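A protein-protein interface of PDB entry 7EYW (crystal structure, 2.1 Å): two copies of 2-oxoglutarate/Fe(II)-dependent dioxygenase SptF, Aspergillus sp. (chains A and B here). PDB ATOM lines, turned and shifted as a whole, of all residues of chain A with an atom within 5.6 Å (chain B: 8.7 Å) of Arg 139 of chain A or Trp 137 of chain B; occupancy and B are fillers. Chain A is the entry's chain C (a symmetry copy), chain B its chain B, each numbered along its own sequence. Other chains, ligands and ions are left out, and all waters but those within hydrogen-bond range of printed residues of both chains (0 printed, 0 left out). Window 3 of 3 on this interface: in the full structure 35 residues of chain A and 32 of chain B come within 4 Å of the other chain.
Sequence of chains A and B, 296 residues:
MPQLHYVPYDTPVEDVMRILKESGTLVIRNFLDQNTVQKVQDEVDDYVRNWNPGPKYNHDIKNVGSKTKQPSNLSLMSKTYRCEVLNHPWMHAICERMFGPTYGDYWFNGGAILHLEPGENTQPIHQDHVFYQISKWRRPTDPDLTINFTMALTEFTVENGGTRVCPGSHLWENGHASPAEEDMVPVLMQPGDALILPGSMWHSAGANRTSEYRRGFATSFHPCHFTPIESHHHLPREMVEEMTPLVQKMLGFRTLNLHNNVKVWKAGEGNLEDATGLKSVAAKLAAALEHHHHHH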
ATOM      1  N   TYR A 103      -9.374 -21.500 -28.301  1.00  0.00           N
ATOM      2  CA  TYR A 103     -10.519 -20.785 -27.757  1.00  0.00           C
ATOM      3  C   TYR A 103     -11.764 -21.642 -27.588  1.00  0.00           C
ATOM      4  O   TYR A 103     -12.724 -21.186 -26.957  1.00  0.00           O
ATOM      5  CB  TYR A 103     -10.861 -19.589 -28.652  1.00  0.00           C
ATOM      6  CG  TYR A 103      -9.767 -18.557 -28.732  1.00  0.00           C
ATOM      7  CD1 TYR A 103      -9.604 -17.611 -27.729  1.00  0.00           C
ATOM      8  CD2 TYR A 103      -8.888 -18.534 -29.806  1.00  0.00           C
ATOM      9  CE1 TYR A 103      -8.604 -16.663 -27.799  1.00  0.00           C
ATOM     10  CE2 TYR A 103      -7.887 -17.591 -29.886  1.00  0.00           C
ATOM     11  CZ  TYR A 103      -7.748 -16.659 -28.879  1.00  0.00           C
ATOM     12  OH  TYR A 103      -6.748 -15.718 -28.954  1.00  0.00           O
ATOM     13  N   ILE A 134      -6.015  -6.231 -27.917  1.00  0.00           N
ATOM     14  CA  ILE A 134      -5.164  -7.359 -27.543  1.00  0.00           C
ATOM     15  C   ILE A 134      -4.269  -7.833 -28.675  1.00  0.00           C
ATOM     16  O   ILE A 134      -3.445  -8.736 -28.467  1.00  0.00           O
ATOM     17  CB  ILE A 134      -6.026  -8.537 -27.046  1.00  0.00           C
ATOM     18  CG1 ILE A 134      -6.958  -9.009 -28.155  1.00  0.00           C
ATOM     19  CG2 ILE A 134      -6.856  -8.124 -25.831  1.00  0.00           C
ATOM     20  CD1 ILE A 134      -7.687 -10.270 -27.822  1.00  0.00           C
ATOM     21  N   SER A 135      -4.395  -7.254 -29.870  1.00  0.00           N
ATOM     22  CA  SER A 135      -3.467  -7.580 -30.945  1.00  0.00           C
ATOM     23  C   SER A 135      -2.067  -7.063 -30.666  1.00  0.00           C
ATOM     24  O   SER A 135      -1.105  -7.581 -31.241  1.00  0.00           O
ATOM     25  CB  SER A 135      -3.970  -7.011 -32.269  1.00  0.00           C
ATOM     26  OG  SER A 135      -3.821  -5.600 -32.305  1.00  0.00           O
ATOM     27  N   TRP A 137      -0.587  -7.393 -27.822  1.00  0.00           N
ATOM     28  CA  TRP A 137       0.035  -8.449 -27.037  1.00  0.00           C
ATOM     29  C   TRP A 137       0.275  -9.715 -27.843  1.00  0.00           C
ATOM     30  O   TRP A 137       1.060 -10.569 -27.413  1.00  0.00           O
ATOM     31  CB  TRP A 137      -0.825  -8.815 -25.822  1.00  0.00           C
ATOM     32  CG  TRP A 137      -1.375  -7.666 -25.027  1.00  0.00           C
ATOM     33  CD1 TRP A 137      -0.973  -6.362 -25.065  1.00  0.00           C
ATOM     34  CD2 TRP A 137      -2.425  -7.733 -24.056  1.00  0.00           C
ATOM     35  NE1 TRP A 137      -1.717  -5.612 -24.185  1.00  0.00           N
ATOM     36  CE2 TRP A 137      -2.613  -6.432 -23.552  1.00  0.00           C
ATOM     37  CE3 TRP A 137      -3.227  -8.770 -23.565  1.00  0.00           C
ATOM     38  CZ2 TRP A 137      -3.570  -6.138 -22.583  1.00  0.00           C
ATOM     39  CZ3 TRP A 137      -4.175  -8.476 -22.604  1.00  0.00           C
ATOM     40  CH2 TRP A 137      -4.338  -7.172 -22.122  1.00  0.00           C
ATOM     41  N   ARG A 138      -0.383  -9.856 -28.989  1.00  0.00           N
ATOM     42  CA  ARG A 138      -0.337 -11.095 -29.750  1.00  0.00           C
ATOM     43  C   ARG A 138       0.975 -11.221 -30.513  1.00  0.00           C
ATOM     44  O   ARG A 138       1.532 -10.229 -30.994  1.00  0.00           O
ATOM     45  CB  ARG A 138      -1.517 -11.157 -30.721  1.00  0.00           C
ATOM     46  CG  ARG A 138      -1.600 -12.434 -31.539  1.00  0.00           C
ATOM     47  CD  ARG A 138      -2.741 -12.374 -32.542  1.00  0.00           C
ATOM     48  NE  ARG A 138      -2.573 -13.349 -33.612  1.00  0.00           N
ATOM     49  CZ  ARG A 138      -1.917 -13.115 -34.742  1.00  0.00           C
ATOM     50  NH1 ARG A 138      -1.359 -11.941 -34.986  1.00  0.00           N
ATOM     51  NH2 ARG A 138      -1.820 -14.084 -35.646  1.00  0.00           N
ATOM     52  N   ARG A 139       1.472 -12.455 -30.611  1.00  0.00           N
ATOM     53  CA  ARG A 139       2.626 -12.871 -31.388  1.00  0.00           C
ATOM     54  C   ARG A 139       2.182 -13.400 -32.746  1.00  0.00           C
ATOM     55  O   ARG A 139       1.087 -13.959 -32.870  1.00  0.00           O
ATOM     56  CB  ARG A 139       3.413 -13.959 -30.649  1.00  0.00           C
ATOM     57  CG  ARG A 139       4.256 -13.444 -29.491  1.00  0.00           C
ATOM     58  CD  ARG A 139       3.530 -13.595 -28.160  1.00  0.00           C
ATOM     59  NE  ARG A 139       3.312 -14.992 -27.802  1.00  0.00           N
ATOM     60  CZ  ARG A 139       2.695 -15.394 -26.699  1.00  0.00           C
ATOM     61  NH1 ARG A 139       2.216 -14.529 -25.820  1.00  0.00           N
ATOM     62  NH2 ARG A 139       2.554 -16.697 -26.472  1.00  0.00           N
ATOM     63  N   PRO A 140       2.998 -13.232 -33.790  1.00  0.00           N
ATOM     64  CA  PRO A 140       2.596 -13.728 -35.119  1.00  0.00           C
ATOM     65  C   PRO A 140       2.367 -15.228 -35.167  1.00  0.00           C
ATOM     66  O   PRO A 140       1.640 -15.700 -36.050  1.00  0.00           O
ATOM     67  CB  PRO A 140       3.765 -13.310 -36.024  1.00  0.00           C
ATOM     68  CG  PRO A 140       4.474 -12.226 -35.279  1.00  0.00           C
ATOM     69  CD  PRO A 140       4.292 -12.530 -33.825  1.00  0.00           C
ATOM     70  N   THR A 141       2.959 -15.992 -34.248  1.00  0.00           N
ATOM     71  CA  THR A 141       2.734 -17.431 -34.200  1.00  0.00           C
ATOM     72  C   THR A 141       1.428 -17.792 -33.505  1.00  0.00           C
ATOM     73  O   THR A 141       0.943 -18.917 -33.669  1.00  0.00           O
ATOM     74  CB  THR A 141       3.906 -18.118 -33.493  1.00  0.00           C
ATOM     75  OG1 THR A 141       5.122 -17.423 -33.800  1.00  0.00           O
ATOM     76  CG2 THR A 141       4.038 -19.562 -33.954  1.00  0.00           C
ATOM     77  N   ASP A 142       0.848 -16.867 -32.741  1.00  0.00           N
ATOM     78  CA  ASP A 142      -0.410 -17.121 -32.063  1.00  0.00           C
ATOM     79  C   ASP A 142      -1.535 -17.302 -33.079  1.00  0.00           C
ATOM     80  O   ASP A 142      -1.422 -16.873 -34.231  1.00  0.00           O
ATOM     81  CB  ASP A 142      -0.742 -15.969 -31.117  1.00  0.00           C
ATOM     82  CG  ASP A 142       0.190 -15.907 -29.923  1.00  0.00           C
ATOM     83  OD1 ASP A 142       0.724 -16.964 -29.527  1.00  0.00           O
ATOM     84  OD2 ASP A 142       0.386 -14.800 -29.378  1.00  0.00           O
ATOM     85  N   PRO A 143      -2.630 -17.951 -32.682  1.00  0.00           N
ATOM     86  CA  PRO A 143      -3.793 -18.033 -33.571  1.00  0.00           C
ATOM     87  C   PRO A 143      -4.349 -16.651 -33.877  1.00  0.00           C
ATOM     88  O   PRO A 143      -4.120 -15.680 -33.152  1.00  0.00           O
ATOM     89  CB  PRO A 143      -4.797 -18.878 -32.775  1.00  0.00           C
ATOM     90  CG  PRO A 143      -3.965 -19.633 -31.792  1.00  0.00           C
ATOM     91  CD  PRO A 143      -2.830 -18.721 -31.441  1.00  0.00           C
ATOM     92  N   LEU A 145      -6.987 -13.559 -34.391  1.00  0.00           N
ATOM     93  CA  LEU A 145      -8.069 -13.020 -33.578  1.00  0.00           C
ATOM     94  C   LEU A 145      -9.402 -13.018 -34.310  1.00  0.00           C
ATOM     95  O   LEU A 145     -10.450 -12.955 -33.659  1.00  0.00           O
ATOM     96  CB  LEU A 145      -7.728 -11.599 -33.127  1.00  0.00           C
ATOM     97  CG  LEU A 145      -6.412 -11.447 -32.363  1.00  0.00           C
ATOM     98  CD1 LEU A 145      -6.115  -9.982 -32.105  1.00  0.00           C
ATOM     99  CD2 LEU A 145      -6.470 -12.219 -31.057  1.00  0.00           C
ATOM    100  N   TYR B 132      -9.585 -16.472 -19.282  1.00  0.00           N
ATOM    101  CA  TYR B 132      -9.265 -15.736 -20.497  1.00  0.00           C
ATOM    102  C   TYR B 132      -7.998 -16.334 -21.094  1.00  0.00           C
ATOM    103  O   TYR B 132      -6.937 -16.304 -20.461  1.00  0.00           O
ATOM    104  CB  TYR B 132      -9.054 -14.248 -20.215  1.00  0.00           C
ATOM    105  CG  TYR B 132     -10.280 -13.485 -19.770  1.00  0.00           C
ATOM    106  CD1 TYR B 132     -11.119 -12.880 -20.696  1.00  0.00           C
ATOM    107  CD2 TYR B 132     -10.588 -13.354 -18.423  1.00  0.00           C
ATOM    108  CE1 TYR B 132     -12.236 -12.174 -20.294  1.00  0.00           C
ATOM    109  CE2 TYR B 132     -11.700 -12.646 -18.011  1.00  0.00           C
ATOM    110  CZ  TYR B 132     -12.523 -12.061 -18.949  1.00  0.00           C
ATOM    111  OH  TYR B 132     -13.634 -11.359 -18.542  1.00  0.00           O
ATOM    112  N   GLN B 133      -8.104 -16.879 -22.308  1.00  0.00           N
ATOM    113  CA  GLN B 133      -6.923 -17.446 -22.949  1.00  0.00           C
ATOM    114  C   GLN B 133      -5.894 -16.374 -23.279  1.00  0.00           C
ATOM    115  O   GLN B 133      -4.696 -16.669 -23.358  1.00  0.00           O
ATOM    116  CB  GLN B 133      -7.323 -18.211 -24.209  1.00  0.00           C
ATOM    117  CG  GLN B 133      -7.349 -19.718 -24.017  1.00  0.00           C
ATOM    118  CD  GLN B 133      -6.019 -20.377 -24.333  1.00  0.00           C
ATOM    119  OE1 GLN B 133      -4.968 -19.738 -24.290  1.00  0.00           O
ATOM    120  NE2 GLN B 133      -6.058 -21.667 -24.647  1.00  0.00           N
ATOM    121  N   ILE B 134      -6.335 -15.125 -23.465  1.00  0.00           N
ATOM    122  CA  ILE B 134      -5.411 -14.027 -23.744  1.00  0.00           C
ATOM    123  C   ILE B 134      -4.674 -13.547 -22.507  1.00  0.00           C
ATOM    124  O   ILE B 134      -3.807 -12.671 -22.620  1.00  0.00           O
ATOM    125  CB  ILE B 134      -6.148 -12.835 -24.388  1.00  0.00           C
ATOM    126  CG1 ILE B 134      -7.269 -12.343 -23.470  1.00  0.00           C
ATOM    127  CG2 ILE B 134      -6.694 -13.222 -25.754  1.00  0.00           C
ATOM    128  CD1 ILE B 134      -8.095 -11.228 -24.070  1.00  0.00           C
ATOM    129  N   SER B 135      -4.993 -14.085 -21.327  1.00  0.00           N
ATOM    130  CA  SER B 135      -4.231 -13.746 -20.132  1.00  0.00           C
ATOM    131  C   SER B 135      -2.793 -14.233 -20.214  1.00  0.00           C
ATOM    132  O   SER B 135      -1.924 -13.679 -19.534  1.00  0.00           O
ATOM    133  CB  SER B 135      -4.905 -14.327 -18.886  1.00  0.00           C
ATOM    134  OG  SER B 135      -4.855 -15.743 -18.894  1.00  0.00           O
ATOM    135  N   LYS B 136      -2.524 -15.256 -21.027  1.00  0.00           N
ATOM    136  CA  LYS B 136      -1.156 -15.717 -21.210  1.00  0.00           C
ATOM    137  C   LYS B 136      -0.343 -14.774 -22.088  1.00  0.00           C
ATOM    138  O   LYS B 136       0.888 -14.759 -21.984  1.00  0.00           O
ATOM    139  CB  LYS B 136      -1.154 -17.130 -21.794  1.00  0.00           C
ATOM    140  CG  LYS B 136      -2.041 -18.104 -21.029  1.00  0.00           C
ATOM    141  CD  LYS B 136      -2.890 -18.943 -21.968  1.00  0.00           C
ATOM    142  CE  LYS B 136      -3.802 -19.890 -21.199  1.00  0.00           C
ATOM    143  NZ  LYS B 136      -4.057 -19.415 -19.812  1.00  0.00           N
ATOM    144  N   TRP B 137      -0.998 -13.989 -22.946  1.00  0.00           N
ATOM    145  CA  TRP B 137      -0.307 -12.927 -23.666  1.00  0.00           C
ATOM    146  C   TRP B 137      -0.103 -11.690 -22.806  1.00  0.00           C
ATOM    147  O   TRP B 137       0.762 -10.865 -23.120  1.00  0.00           O
ATOM    148  CB  TRP B 137      -1.084 -12.518 -24.922  1.00  0.00           C
ATOM    149  CG  TRP B 137      -1.545 -13.638 -25.809  1.00  0.00           C
ATOM    150  CD1 TRP B 137      -1.166 -14.949 -25.760  1.00  0.00           C
ATOM    151  CD2 TRP B 137      -2.475 -13.531 -26.891  1.00  0.00           C
ATOM    152  NE1 TRP B 137      -1.809 -15.664 -26.741  1.00  0.00           N
ATOM    153  CE2 TRP B 137      -2.619 -14.816 -27.451  1.00  0.00           C
ATOM    154  CE3 TRP B 137      -3.204 -12.471 -27.441  1.00  0.00           C
ATOM    155  CZ2 TRP B 137      -3.458 -15.068 -28.532  1.00  0.00           C
ATOM    156  CZ3 TRP B 137      -4.035 -12.723 -28.512  1.00  0.00           C
ATOM    157  CH2 TRP B 137      -4.157 -14.011 -29.048  1.00  0.00           C
ATOM    158  N   ARG B 138      -0.880 -11.547 -21.739  1.00  0.00           N
ATOM    159  CA  ARG B 138      -0.851 -10.343 -20.925  1.00  0.00           C
ATOM    160  C   ARG B 138       0.421 -10.284 -20.088  1.00  0.00           C
ATOM    161  O   ARG B 138       1.029 -11.307 -19.762  1.00  0.00           O
ATOM    162  CB  ARG B 138      -2.083 -10.293 -20.020  1.00  0.00           C
ATOM    163  CG  ARG B 138      -2.351  -8.947 -19.373  1.00  0.00           C
ATOM    164  CD  ARG B 138      -3.541  -9.021 -18.434  1.00  0.00           C
ATOM    165  NE  ARG B 138      -3.453  -8.027 -17.372  1.00  0.00           N
ATOM    166  CZ  ARG B 138      -2.865  -8.233 -16.200  1.00  0.00           C
ATOM    167  NH1 ARG B 138      -2.309  -9.395 -15.901  1.00  0.00           N
ATOM    168  NH2 ARG B 138      -2.837  -7.248 -15.307  1.00  0.00           N
ATOM    169  N   ARG B 139       0.825  -9.065 -19.748  1.00  0.00           N
ATOM    170  CA  ARG B 139       1.934  -8.838 -18.842  1.00  0.00           C
ATOM    171  C   ARG B 139       1.445  -8.053 -17.629  1.00  0.00           C
ATOM    172  O   ARG B 139       0.519  -7.243 -17.746  1.00  0.00           O
ATOM    173  CB  ARG B 139       3.067  -8.082 -19.545  1.00  0.00           C
ATOM    174  CG  ARG B 139       3.732  -8.926 -20.616  1.00  0.00           C
ATOM    175  CD  ARG B 139       5.245  -8.939 -20.505  1.00  0.00           C
ATOM    176  NE  ARG B 139       5.715  -9.985 -19.603  1.00  0.00           N
ATOM    177  CZ  ARG B 139       6.541  -9.779 -18.587  1.00  0.00           C
ATOM    178  NH1 ARG B 139       7.081  -8.593 -18.366  1.00  0.00           N
ATOM    179  NH2 ARG B 139       6.840 -10.792 -17.778  1.00  0.00           N
ATOM    180  N   PRO B 140       2.032  -8.282 -16.450  1.00  0.00           N
ATOM    181  CA  PRO B 140       1.475  -7.688 -15.220  1.00  0.00           C
ATOM    182  C   PRO B 140       1.390  -6.168 -15.237  1.00  0.00           C
ATOM    183  O   PRO B 140       0.689  -5.601 -14.389  1.00  0.00           O
ATOM    184  CB  PRO B 140       2.432  -8.179 -14.125  1.00  0.00           C
ATOM    185  CG  PRO B 140       3.088  -9.393 -14.701  1.00  0.00           C
ATOM    186  CD  PRO B 140       3.200  -9.133 -16.172  1.00  0.00           C
ATOM    187  N   ASP B 142       0.153  -4.584 -17.875  1.00  0.00           N
ATOM    188  CA  ASP B 142      -1.010  -4.299 -18.698  1.00  0.00           C
ATOM    189  C   ASP B 142      -2.252  -4.154 -17.825  1.00  0.00           C
ATOM    190  O   ASP B 142      -2.301  -4.674 -16.707  1.00  0.00           O
ATOM    191  CB  ASP B 142      -1.213  -5.414 -19.719  1.00  0.00           C
ATOM    192  CG  ASP B 142      -0.121  -5.449 -20.768  1.00  0.00           C
ATOM    193  OD1 ASP B 142       0.385  -4.368 -21.136  1.00  0.00           O
ATOM    194  OD2 ASP B 142       0.232  -6.557 -21.223  1.00  0.00           O
ATOM    195  N   LEU B 145      -7.868  -7.824 -17.210  1.00  0.00           N
ATOM    196  CA  LEU B 145      -8.863  -8.329 -18.145  1.00  0.00           C
ATOM    197  C   LEU B 145     -10.270  -8.302 -17.570  1.00  0.00           C
ATOM    198  O   LEU B 145     -11.238  -8.410 -18.330  1.00  0.00           O
ATOM    199  CB  LEU B 145      -8.511  -9.755 -18.566  1.00  0.00           C
ATOM    200  CG  LEU B 145      -7.175  -9.925 -19.287  1.00  0.00           C
ATOM    201  CD1 LEU B 145      -6.916 -11.389 -19.561  1.00  0.00           C
ATOM    202  CD2 LEU B 145      -7.158  -9.127 -20.580  1.00  0.00           C
ATOM    203  N   ASN B 174       3.509 -14.342 -15.622  1.00  0.00           N
ATOM    204  CA  ASN B 174       2.665 -15.441 -16.072  1.00  0.00           C
ATOM    205  C   ASN B 174       3.343 -16.777 -15.799  1.00  0.00           C
ATOM    206  O   ASN B 174       4.543 -16.946 -16.037  1.00  0.00           O
ATOM    207  CB  ASN B 174       2.359 -15.304 -17.563  1.00  0.00           C
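Ile 134 of chain A touches Ile 134 of chain B (CD1 to CG2, 3.7 Å). Trp 137 of chain B touches Ile 134 of chain A. Trp 137 of chain B touches Trp 137 of chain A (O to CB, 3.7 Å). Trp 137 of chain A touches Arg 138 of chain B. Asp 142 of chain B touches Trp 137 of chain A (OD2 to NE1, 3.7 Å). Trp 137 of chain A touches Leu 145 of chain B. Trp 137 of chain B touches Arg 138 of chain A. Arg 139 of chain A touches Trp 137 of chain B. Trp 137 of chain B touches Asp 142 of chain A. CD2 of Leu 145 of chain A touches CH2 of Trp 137 of chain B, 3.5 Å away.
The backbone NH of Arg 139 of chain B is in hydrogen-bond range of the side-chain carboxylate of Asp 142 of chain B (3.0 Å). NH2 of Arg 138 of chain A sits at hydrogen-bond distance from O of Asp 142 of chain A (3.2 Å). The backbone carbonyl oxygen (O) of Pro 143 of chain A sits at hydrogen-bond distance from the guanidinium group (NE) of Arg 138 of chain A (2.8 Å). The guanidinium group of Arg 139 of chain A is in salt-bridge range of the side-chain carboxylate of Asp 142 of chain A (3.3 Å). The guanidinium group (NH2) of Arg 138 of chain B sits at hydrogen-bond distance from the backbone carbonyl oxygen (O) of Asp 142 of chain B.
Printed residues of chain B that touch a printed residue of chain A: Ile 134, Trp 137, Arg 138, Asp 142 and Leu 145. Hydrophobic or aromatic side chains of chain B within 4 Å of the printed part of chain A: Ile 134, Trp 137 and Leu 145. Hydrophobic or aromatic side chains of chain A that line the printed part of chain B: Tyr 103, Ile 134, Trp 137 and Leu 145.
Of chain B, only Trp 137 (3.7 Å) comes within 4 Å of Arg 138 of chain A. Arg 139 of chain A touches just one residue of chain B: Trp 137 (3.4 Å). No residue of chain B comes within 4 Å of Pro 140 of chain A. Printed residues of chain A within 4 Å of Ile 134 of chain B: Ile 134 (3.7 Å). Of chain A, only Tyr 103 (3.1 Å), Ile 134 (3.9 Å), Trp 137 (3.7 Å), Arg 138 (3.7 Å), Arg 139 (3.4 Å), Asp 142 (3.5 Å) and Leu 145 (3.5 Å) come within 4 Å of Trp 137 of chain B. Printed residues of chain A within 4 Å of Asp 142 of chain B: Trp 137 (3.7 Å). Asn 174 of chain B touches none of the printed residues of chain A. The nearest residue of chain B that does not touch Arg 139 of chain A is Lys 136 of chain B (4.1 Å). The nearest residue of chain A that does not touch Trp 137 of chain B is Pro 143 of chain A (4.4 Å). The nearest printed residue of chain A that does not touch Asp 142 of chain B is Ile 134 of chain A (8.3 Å).
Ile 134 of chain A touches Trp 137 of chain B, but with the chains exchanged Trp 137 of chain A does not touch Ile 134 of chain B (4.1 Å). Trp 137 of chain A touches Arg 138 of chain B, and with the chains exchanged Arg 138 of chain A touches Trp 137 of chain B. Trp 137 of chain A touches Asp 142 of chain B, and with the chains exchanged Asp 142 of chain A touches Trp 137 of chain B. Trp 137 of chain A touches Leu 145 of chain B, and with the chains exchanged Leu 145 of chain A touches Trp 137 of chain B. Positions printed for both chains: 134, 135, 137, 138, 139, 140, 142 and 145. Of the 11 pairs that touch across the chains among the printed residues, 8 have their exchanged pair printed and touching as well.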
